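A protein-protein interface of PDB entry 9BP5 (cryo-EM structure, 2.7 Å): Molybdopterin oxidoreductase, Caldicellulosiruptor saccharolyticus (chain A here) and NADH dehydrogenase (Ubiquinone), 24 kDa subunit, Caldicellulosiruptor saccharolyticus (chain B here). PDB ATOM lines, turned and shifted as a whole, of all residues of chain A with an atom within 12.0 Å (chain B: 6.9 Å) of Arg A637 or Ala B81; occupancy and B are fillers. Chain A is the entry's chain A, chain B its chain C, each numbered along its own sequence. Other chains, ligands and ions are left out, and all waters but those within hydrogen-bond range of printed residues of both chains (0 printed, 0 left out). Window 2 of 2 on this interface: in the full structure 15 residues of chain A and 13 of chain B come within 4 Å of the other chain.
NE of Arg A637 is in hydrogen-bond range of O of Phe B79 (2.7 Å). The backbone NH (N) of Asn A636 is in hydrogen-bond range of the side-chain hydroxyl (OG1) of Thr B78, at 2.8 Å. NH2 of Arg A637 lies close to N of Ala B81.
The backbone NH (N) of Val A635 lies within hydrogen-bond range of the backbone carbonyl oxygen (O) of Ile A642 (2.8 Å). The side-chain amide nitrogen of Asn A636 sits at hydrogen-bond distance from the backbone carbonyl oxygen of Glu A640, 2.9 Å away.
Among the printed residues, merely in contact across the chains: Val A635 with Thr B78, Arg A637 with Tyr B80 and Phe A634 with Thr B78.
Arg A637 touches three residues of chain B. Phe B79 touches just one residue of chain A: Arg A637. No residue of chain A comes within 4 Å of Gln B82. Phe B83 touches none of the printed residues of chain A. Of the printed residues of chain B, Asn A636 touches Thr B78 (2.8 Å). Printed residues of chain B within 4 Å of Val A635: Thr B78. Of the printed residues of chain B, Phe A634 touches Thr B78 (3.98 Å). Printed residues of chain A within 4 Å of Thr B78: Phe A634 (3.98 Å), Val A635 (3.2 Å) and Asn A636 (2.8 Å). Printed residues of chain A within 4 Å of Tyr B80: Arg A637 (3.7 Å). The nearest residue of chain B that does not touch Arg A637 is Thr B78 (4.1 Å). The nearest printed residue of chain B that does not touch Val A635 is Phe B79 (5.8 Å).
Hydrophobic or aromatic side chains of chain B within 4 Å of the printed part of chain A: Phe B79 and Ala B81. Hydrophobic or aromatic side chains of chain A within 4 Å of the printed part of chain B: Val A635. Among the printed residues, 6 pairs touch across the chains. Among the printed residues, no Asp or Glu carboxylate lies within 4 Å of a Lys or Arg side-chain nitrogen of the other chain.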
ATOM      1  N   TYR A  44      35.048  11.582  26.864  1.00  0.00           N
ATOM      2  CA  TYR A  44      33.660  11.162  26.747  1.00  0.00           C
ATOM      3  C   TYR A  44      33.404   9.762  27.281  1.00  0.00           C
ATOM      4  O   TYR A  44      32.343   9.514  27.853  1.00  0.00           O
ATOM      5  CB  TYR A  44      33.234  11.237  25.283  1.00  0.00           C
ATOM      6  CG  TYR A  44      31.748  11.284  25.057  1.00  0.00           C
ATOM      7  CD1 TYR A  44      30.959  12.231  25.683  1.00  0.00           C
ATOM      8  CD2 TYR A  44      31.139  10.393  24.198  1.00  0.00           C
ATOM      9  CE1 TYR A  44      29.608  12.274  25.469  1.00  0.00           C
ATOM     10  CE2 TYR A  44      29.790  10.427  23.982  1.00  0.00           C
ATOM     11  CZ  TYR A  44      29.029  11.368  24.615  1.00  0.00           C
ATOM     12  OH  TYR A  44      27.676  11.395  24.390  1.00  0.00           O
ATOM     13  N   GLU A  95      24.746  -3.380  15.825  1.00  0.00           N
ATOM     14  CA  GLU A  95      23.800  -2.392  15.326  1.00  0.00           C
ATOM     15  C   GLU A  95      24.274  -1.731  14.037  1.00  0.00           C
ATOM     16  O   GLU A  95      23.931  -0.575  13.774  1.00  0.00           O
ATOM     17  CB  GLU A  95      23.539  -1.337  16.398  1.00  0.00           C
ATOM     18  CG  GLU A  95      24.755  -1.010  17.237  1.00  0.00           C
ATOM     19  CD  GLU A  95      24.688   0.374  17.850  1.00  0.00           C
ATOM     20  OE1 GLU A  95      23.581   0.800  18.237  1.00  0.00           O
ATOM     21  OE2 GLU A  95      25.742   1.039  17.937  1.00  0.00           O
ATOM     22  N   TYR A 593      17.749  -7.384  16.793  1.00  0.00           N
ATOM     23  CA  TYR A 593      17.107  -6.221  16.204  1.00  0.00           C
ATOM     24  C   TYR A 593      18.144  -5.186  15.797  1.00  0.00           C
ATOM     25  O   TYR A 593      19.067  -4.875  16.552  1.00  0.00           O
ATOM     26  CB  TYR A 593      16.111  -5.603  17.180  1.00  0.00           C
ATOM     27  CG  TYR A 593      15.385  -4.421  16.591  1.00  0.00           C
ATOM     28  CD1 TYR A 593      14.471  -4.590  15.564  1.00  0.00           C
ATOM     29  CD2 TYR A 593      15.628  -3.133  17.045  1.00  0.00           C
ATOM     30  CE1 TYR A 593      13.814  -3.515  15.016  1.00  0.00           C
ATOM     31  CE2 TYR A 593      14.974  -2.052  16.501  1.00  0.00           C
ATOM     32  CZ  TYR A 593      14.067  -2.249  15.487  1.00  0.00           C
ATOM     33  OH  TYR A 593      13.407  -1.174  14.939  1.00  0.00           O
ATOM     34  N   HIS A 595      18.343  -1.298  13.804  1.00  0.00           N
ATOM     35  CA  HIS A 595      17.641  -0.158  13.237  1.00  0.00           C
ATOM     36  C   HIS A 595      17.930  -0.041  11.746  1.00  0.00           C
ATOM     37  O   HIS A 595      19.002  -0.411  11.267  1.00  0.00           O
ATOM     38  CB  HIS A 595      18.060   1.135  13.935  1.00  0.00           C
ATOM     39  CG  HIS A 595      17.514   1.291  15.319  1.00  0.00           C
ATOM     40  ND1 HIS A 595      16.166   1.409  15.579  1.00  0.00           N
ATOM     41  CD2 HIS A 595      18.136   1.384  16.517  1.00  0.00           C
ATOM     42  CE1 HIS A 595      15.981   1.551  16.878  1.00  0.00           C
ATOM     43  NE2 HIS A 595      17.161   1.541  17.469  1.00  0.00           N
ATOM     44  N   ARG A 597      17.225   3.297   9.724  1.00  0.00           N
ATOM     45  CA  ARG A 597      16.692   4.652   9.762  1.00  0.00           C
ATOM     46  C   ARG A 597      17.364   5.571   8.750  1.00  0.00           C
ATOM     47  O   ARG A 597      17.257   6.794   8.866  1.00  0.00           O
ATOM     48  CB  ARG A 597      16.825   5.236  11.168  1.00  0.00           C
ATOM     49  CG  ARG A 597      16.486   4.268  12.272  1.00  0.00           C
ATOM     50  CD  ARG A 597      16.530   4.942  13.621  1.00  0.00           C
ATOM     51  NE  ARG A 597      17.829   4.793  14.262  1.00  0.00           N
ATOM     52  CZ  ARG A 597      18.088   5.146  15.513  1.00  0.00           C
ATOM     53  NH1 ARG A 597      17.157   5.674  16.287  1.00  0.00           N
ATOM     54  NH2 ARG A 597      19.313   4.967  15.994  1.00  0.00           N
ATOM     55  N   LEU A 615      27.680   6.034  17.641  1.00  0.00           N
ATOM     56  CA  LEU A 615      27.247   6.906  18.732  1.00  0.00           C
ATOM     57  C   LEU A 615      28.408   7.298  19.638  1.00  0.00           C
ATOM     58  O   LEU A 615      28.287   7.313  20.863  1.00  0.00           O
ATOM     59  CB  LEU A 615      26.116   6.266  19.534  1.00  0.00           C
ATOM     60  CG  LEU A 615      24.738   6.373  18.883  1.00  0.00           C
ATOM     61  CD1 LEU A 615      23.713   5.609  19.676  1.00  0.00           C
ATOM     62  CD2 LEU A 615      24.328   7.821  18.737  1.00  0.00           C
ATOM     63  N   ILE A 620      28.714  15.792  17.343  1.00  0.00           N
ATOM     64  CA  ILE A 620      28.037  16.724  18.238  1.00  0.00           C
ATOM     65  C   ILE A 620      29.056  17.523  19.031  1.00  0.00           C
ATOM     66  O   ILE A 620      28.964  18.751  19.150  1.00  0.00           O
ATOM     67  CB  ILE A 620      27.086  15.959  19.176  1.00  0.00           C
ATOM     68  CG1 ILE A 620      26.053  15.175  18.377  1.00  0.00           C
ATOM     69  CG2 ILE A 620      26.424  16.898  20.161  1.00  0.00           C
ATOM     70  CD1 ILE A 620      25.587  13.937  19.068  1.00  0.00           C
ATOM     71  N   GLY A 633      22.647  17.088  17.580  1.00  0.00           N
ATOM     72  CA  GLY A 633      22.381  16.660  18.939  1.00  0.00           C
ATOM     73  C   GLY A 633      21.886  15.234  18.980  1.00  0.00           C
ATOM     74  O   GLY A 633      21.574  14.623  17.956  1.00  0.00           O
ATOM     75  N   PHE A 634      21.831  14.706  20.199  1.00  0.00           N
ATOM     76  CA  PHE A 634      21.265  13.388  20.434  1.00  0.00           C
ATOM     77  C   PHE A 634      19.749  13.473  20.484  1.00  0.00           C
ATOM     78  O   PHE A 634      19.183  14.427  21.015  1.00  0.00           O
ATOM     79  CB  PHE A 634      21.788  12.800  21.742  1.00  0.00           C
ATOM     80  CG  PHE A 634      23.188  12.278  21.660  1.00  0.00           C
ATOM     81  CD1 PHE A 634      23.509  11.255  20.792  1.00  0.00           C
ATOM     82  CD2 PHE A 634      24.181  12.804  22.462  1.00  0.00           C
ATOM     83  CE1 PHE A 634      24.796  10.771  20.718  1.00  0.00           C
ATOM     84  CE2 PHE A 634      25.467  12.325  22.390  1.00  0.00           C
ATOM     85  CZ  PHE A 634      25.774  11.306  21.517  1.00  0.00           C
ATOM     86  N   VAL A 635      19.093  12.471  19.917  1.00  0.00           N
ATOM     87  CA  VAL A 635      17.644  12.353  19.923  1.00  0.00           C
ATOM     88  C   VAL A 635      17.302  10.962  20.433  1.00  0.00           C
ATOM     89  O   VAL A 635      18.042  10.000  20.205  1.00  0.00           O
ATOM     90  CB  VAL A 635      17.043  12.610  18.523  1.00  0.00           C
ATOM     91  CG1 VAL A 635      15.531  12.529  18.547  1.00  0.00           C
ATOM     92  CG2 VAL A 635      17.483  13.961  18.007  1.00  0.00           C
ATOM     93  N   ASN A 636      16.183  10.871  21.154  1.00  0.00           N
ATOM     94  CA  ASN A 636      15.720   9.657  21.819  1.00  0.00           C
ATOM     95  C   ASN A 636      16.668   9.275  22.944  1.00  0.00           C
ATOM     96  O   ASN A 636      17.493  10.087  23.369  1.00  0.00           O
ATOM     97  CB  ASN A 636      15.562   8.499  20.832  1.00  0.00           C
ATOM     98  CG  ASN A 636      14.658   8.836  19.679  1.00  0.00           C
ATOM     99  OD1 ASN A 636      13.659   9.528  19.846  1.00  0.00           O
ATOM    100  ND2 ASN A 636      14.999   8.350  18.500  1.00  0.00           N
ATOM    101  N   ARG A 637      16.554   8.049  23.440  1.00  0.00           N
ATOM    102  CA  ARG A 637      17.333   7.644  24.597  1.00  0.00           C
ATOM    103  C   ARG A 637      17.499   6.133  24.572  1.00  0.00           C
ATOM    104  O   ARG A 637      16.540   5.404  24.312  1.00  0.00           O
ATOM    105  CB  ARG A 637      16.651   8.103  25.892  1.00  0.00           C
ATOM    106  CG  ARG A 637      17.369   7.728  27.158  1.00  0.00           C
ATOM    107  CD  ARG A 637      16.409   7.110  28.153  1.00  0.00           C
ATOM    108  NE  ARG A 637      15.513   8.096  28.744  1.00  0.00           N
ATOM    109  CZ  ARG A 637      14.578   7.814  29.639  1.00  0.00           C
ATOM    110  NH1 ARG A 637      14.373   6.576  30.056  1.00  0.00           N
ATOM    111  NH2 ARG A 637      13.829   8.797  30.128  1.00  0.00           N
ATOM    112  N   GLY A 638      18.719   5.675  24.830  1.00  0.00           N
ATOM    113  CA  GLY A 638      19.000   4.256  24.918  1.00  0.00           C
ATOM    114  C   GLY A 638      19.327   3.612  23.593  1.00  0.00           C
ATOM    115  O   GLY A 638      20.135   4.132  22.821  1.00  0.00           O
ATOM    116  N   PHE A 639      18.707   2.464  23.325  1.00  0.00           N
ATOM    117  CA  PHE A 639      18.894   1.802  22.043  1.00  0.00           C
ATOM    118  C   PHE A 639      18.338   2.622  20.888  1.00  0.00           C
ATOM    119  O   PHE A 639      18.754   2.420  19.744  1.00  0.00           O
ATOM    120  CB  PHE A 639      18.241   0.421  22.072  1.00  0.00           C
ATOM    121  CG  PHE A 639      18.730  -0.502  21.001  1.00  0.00           C
ATOM    122  CD1 PHE A 639      19.994  -1.049  21.067  1.00  0.00           C
ATOM    123  CD2 PHE A 639      17.921  -0.826  19.928  1.00  0.00           C
ATOM    124  CE1 PHE A 639      20.443  -1.896  20.085  1.00  0.00           C
ATOM    125  CE2 PHE A 639      18.367  -1.672  18.942  1.00  0.00           C
ATOM    126  CZ  PHE A 639      19.629  -2.206  19.020  1.00  0.00           C
ATOM    127  N   GLU A 640      17.419   3.542  21.159  1.00  0.00           N
ATOM    128  CA  GLU A 640      16.810   4.366  20.126  1.00  0.00           C
ATOM    129  C   GLU A 640      17.579   5.647  19.859  1.00  0.00           C
ATOM    130  O   GLU A 640      17.135   6.455  19.042  1.00  0.00           O
ATOM    131  CB  GLU A 640      15.372   4.713  20.512  1.00  0.00           C
ATOM    132  CG  GLU A 640      14.560   3.524  20.956  1.00  0.00           C
ATOM    133  CD  GLU A 640      14.112   2.669  19.795  1.00  0.00           C
ATOM    134  OE1 GLU A 640      14.039   3.196  18.666  1.00  0.00           O
ATOM    135  OE2 GLU A 640      13.835   1.471  20.008  1.00  0.00           O
ATOM    136  N   THR A 641      18.710   5.851  20.526  1.00  0.00           N
ATOM    137  CA  THR A 641      19.452   7.093  20.384  1.00  0.00           C
ATOM    138  C   THR A 641      19.933   7.262  18.952  1.00  0.00           C
ATOM    139  O   THR A 641      20.451   6.325  18.341  1.00  0.00           O
ATOM    140  CB  THR A 641      20.640   7.111  21.344  1.00  0.00           C
ATOM    141  OG1 THR A 641      20.208   6.706  22.645  1.00  0.00           O
ATOM    142  CG2 THR A 641      21.216   8.505  21.438  1.00  0.00           C
ATOM    143  N   ILE A 642      19.753   8.466  18.417  1.00  0.00           N
ATOM    144  CA  ILE A 642      20.199   8.810  17.077  1.00  0.00           C
ATOM    145  C   ILE A 642      20.846  10.185  17.154  1.00  0.00           C
ATOM    146  O   ILE A 642      20.661  10.927  18.117  1.00  0.00           O
ATOM    147  CB  ILE A 642      19.026   8.778  16.065  1.00  0.00           C
ATOM    148  CG1 ILE A 642      19.527   8.700  14.623  1.00  0.00           C
ATOM    149  CG2 ILE A 642      18.096   9.959  16.265  1.00  0.00           C
ATOM    150  CD1 ILE A 642      18.432   8.498  13.624  1.00  0.00           C
ATOM    151  N   VAL A 643      21.652  10.509  16.154  1.00  0.00           N
ATOM    152  CA  VAL A 643      22.227  11.842  16.028  1.00  0.00           C
ATOM    153  C   VAL A 643      21.463  12.556  14.928  1.00  0.00           C
ATOM    154  O   VAL A 643      21.352  12.046  13.808  1.00  0.00           O
ATOM    155  CB  VAL A 643      23.732  11.793  15.724  1.00  0.00           C
ATOM    156  CG1 VAL A 643      24.268  13.192  15.531  1.00  0.00           C
ATOM    157  CG2 VAL A 643      24.470  11.106  16.848  1.00  0.00           C
ATOM    158  N   LYS A 644      20.916  13.722  15.244  1.00  0.00           N
ATOM    159  CA  LYS A 644      20.095  14.437  14.288  1.00  0.00           C
ATOM    160  C   LYS A 644      20.437  15.915  14.323  1.00  0.00           C
ATOM    161  O   LYS A 644      20.890  16.428  15.352  1.00  0.00           O
ATOM    162  CB  LYS A 644      18.601  14.246  14.584  1.00  0.00           C
ATOM    163  CG  LYS A 644      17.970  13.079  13.857  1.00  0.00           C
ATOM    164  CD  LYS A 644      16.521  12.910  14.256  1.00  0.00           C
ATOM    165  CE  LYS A 644      15.856  11.808  13.458  1.00  0.00           C
ATOM    166  NZ  LYS A 644      14.574  11.374  14.076  1.00  0.00           N
ATOM    167  N   GLN B  48       4.727  21.760  28.299  1.00  0.00           N
ATOM    168  CA  GLN B  48       3.890  20.572  28.202  1.00  0.00           C
ATOM    169  C   GLN B  48       2.618  20.730  29.020  1.00  0.00           C
ATOM    170  O   GLN B  48       1.558  20.228  28.633  1.00  0.00           O
ATOM    171  CB  GLN B  48       4.670  19.341  28.654  1.00  0.00           C
ATOM    172  CG  GLN B  48       3.935  18.042  28.436  1.00  0.00           C
ATOM    173  CD  GLN B  48       4.868  16.864  28.370  1.00  0.00           C
ATOM    174  OE1 GLN B  48       5.311  16.471  27.294  1.00  0.00           O
ATOM    175  NE2 GLN B  48       5.179  16.290  29.524  1.00  0.00           N
ATOM    176  N   ILE B  76      16.923  17.299  24.906  1.00  0.00           N
ATOM    177  CA  ILE B  76      16.249  17.201  26.196  1.00  0.00           C
ATOM    178  C   ILE B  76      14.826  16.696  26.013  1.00  0.00           C
ATOM    179  O   ILE B  76      14.346  15.856  26.782  1.00  0.00           O
ATOM    180  CB  ILE B  76      16.272  18.552  26.928  1.00  0.00           C
ATOM    181  CG1 ILE B  76      17.699  19.061  27.070  1.00  0.00           C
ATOM    182  CG2 ILE B  76      15.640  18.415  28.290  1.00  0.00           C
ATOM    183  CD1 ILE B  76      17.774  20.542  27.296  1.00  0.00           C
ATOM    184  N   ALA B  77      14.125  17.196  24.991  1.00  0.00           N
ATOM    185  CA  ALA B  77      12.734  16.814  24.798  1.00  0.00           C
ATOM    186  C   ALA B  77      12.594  15.338  24.467  1.00  0.00           C
ATOM    187  O   ALA B  77      11.597  14.713  24.842  1.00  0.00           O
ATOM    188  CB  ALA B  77      12.105  17.665  23.698  1.00  0.00           C
ATOM    189  N   THR B  78      13.560  14.765  23.763  1.00  0.00           N
ATOM    190  CA  THR B  78      13.493  13.357  23.406  1.00  0.00           C
ATOM    191  C   THR B  78      14.238  12.454  24.382  1.00  0.00           C
ATOM    192  O   THR B  78      14.176  11.230  24.236  1.00  0.00           O
ATOM    193  CB  THR B  78      14.035  13.150  21.988  1.00  0.00           C
ATOM    194  OG1 THR B  78      15.425  13.491  21.952  1.00  0.00           O
ATOM    195  CG2 THR B  78      13.283  14.023  21.000  1.00  0.00           C
ATOM    196  N   PHE B  79      14.937  13.017  25.371  1.00  0.00           N
ATOM    197  CA  PHE B  79      15.647  12.177  26.329  1.00  0.00           C
ATOM    198  C   PHE B  79      14.735  11.692  27.446  1.00  0.00           C
ATOM    199  O   PHE B  79      14.841  10.539  27.877  1.00  0.00           O
ATOM    200  CB  PHE B  79      16.837  12.935  26.922  1.00  0.00           C
ATOM    201  CG  PHE B  79      17.645  12.128  27.905  1.00  0.00           C
ATOM    202  CD1 PHE B  79      18.618  11.251  27.468  1.00  0.00           C
ATOM    203  CD2 PHE B  79      17.434  12.253  29.264  1.00  0.00           C
ATOM    204  CE1 PHE B  79      19.359  10.515  28.364  1.00  0.00           C
ATOM    205  CE2 PHE B  79      18.174  11.515  30.162  1.00  0.00           C
ATOM    206  CZ  PHE B  79      19.136  10.647  29.709  1.00  0.00           C
ATOM    207  N   TYR B  80      13.843  12.545  27.926  1.00  0.00           N
ATOM    208  CA  TYR B  80      13.063  12.259  29.117  1.00  0.00           C
ATOM    209  C   TYR B  80      11.712  11.658  28.756  1.00  0.00           C
ATOM    210  O   TYR B  80      11.121  11.981  27.724  1.00  0.00           O
ATOM    211  CB  TYR B  80      12.878  13.525  29.950  1.00  0.00           C
ATOM    212  CG  TYR B  80      14.175  14.042  30.522  1.00  0.00           C
ATOM    213  CD1 TYR B  80      14.811  13.377  31.556  1.00  0.00           C
ATOM    214  CD2 TYR B  80      14.771  15.183  30.016  1.00  0.00           C
ATOM    215  CE1 TYR B  80      15.999  13.840  32.076  1.00  0.00           C
ATOM    216  CE2 TYR B  80      15.959  15.652  30.530  1.00  0.00           C
ATOM    217  CZ  TYR B  80      16.568  14.977  31.558  1.00  0.00           C
ATOM    218  OH  TYR B  80      17.752  15.446  32.071  1.00  0.00           O
ATOM    219  N   ALA B  81      11.234  10.765  29.623  1.00  0.00           N
ATOM    220  CA  ALA B  81       9.993  10.049  29.359  1.00  0.00           C
ATOM    221  C   ALA B  81       8.764  10.921  29.566  1.00  0.00           C
ATOM    222  O   ALA B  81       7.725  10.672  28.945  1.00  0.00           O
ATOM    223  CB  ALA B  81       9.905   8.809  30.248  1.00  0.00           C
ATOM    224  N   GLN B  82       8.853  11.933  30.429  1.00  0.00           N
ATOM    225  CA  GLN B  82       7.710  12.804  30.669  1.00  0.00           C
ATOM    226  C   GLN B  82       7.325  13.608  29.437  1.00  0.00           C
ATOM    227  O   GLN B  82       6.177  14.049  29.333  1.00  0.00           O
ATOM    228  CB  GLN B  82       8.006  13.751  31.830  1.00  0.00           C
ATOM    229  CG  GLN B  82       6.791  14.489  32.360  1.00  0.00           C
ATOM    230  CD  GLN B  82       7.153  15.563  33.362  1.00  0.00           C
ATOM    231  OE1 GLN B  82       8.135  16.282  33.189  1.00  0.00           O
ATOM    232  NE2 GLN B  82       6.359  15.679  34.418  1.00  0.00           N
ATOM    233  N   PHE B  83       8.248  13.800  28.501  1.00  0.00           N
ATOM    234  CA  PHE B  83       8.015  14.650  27.344  1.00  0.00           C
ATOM    235  C   PHE B  83       7.464  13.832  26.186  1.00  0.00           C
ATOM    236  O   PHE B  83       8.011  12.779  25.845  1.00  0.00           O
ATOM    237  CB  PHE B  83       9.309  15.346  26.931  1.00  0.00           C
ATOM    238  CG  PHE B  83       9.877  16.230  27.993  1.00  0.00           C
ATOM    239  CD1 PHE B  83       9.048  16.994  28.785  1.00  0.00           C
ATOM    240  CD2 PHE B  83      11.237  16.295  28.202  1.00  0.00           C
ATOM    241  CE1 PHE B  83       9.563  17.806  29.760  1.00  0.00           C
ATOM    242  CE2 PHE B  83      11.755  17.106  29.176  1.00  0.00           C
ATOM    243  CZ  PHE B  83      10.917  17.862  29.956  1.00  0.00           C
ATOM    244  N   ARG B  84       6.385  14.322  25.584  1.00  0.00           N
ATOM    245  CA  ARG B  84       5.732  13.658  24.466  1.00  0.00           C
ATOM    246  C   ARG B  84       5.647  14.627  23.300  1.00  0.00           C
ATOM    247  O   ARG B  84       5.204  15.767  23.469  1.00  0.00           O
ATOM    248  CB  ARG B  84       4.335  13.173  24.858  1.00  0.00           C
ATOM    249  CG  ARG B  84       3.548  14.168  25.693  1.00  0.00           C
ATOM    250  CD  ARG B  84       2.852  13.489  26.859  1.00  0.00           C
ATOM    251  NE  ARG B  84       1.890  14.369  27.511  1.00  0.00           N
ATOM    252  CZ  ARG B  84       1.368  14.150  28.709  1.00  0.00           C
ATOM    253  NH1 ARG B  84       1.695  13.084  29.421  1.00  0.00           N
ATOM    254  NH2 ARG B  84       0.496  15.022  29.206  1.00  0.00           N
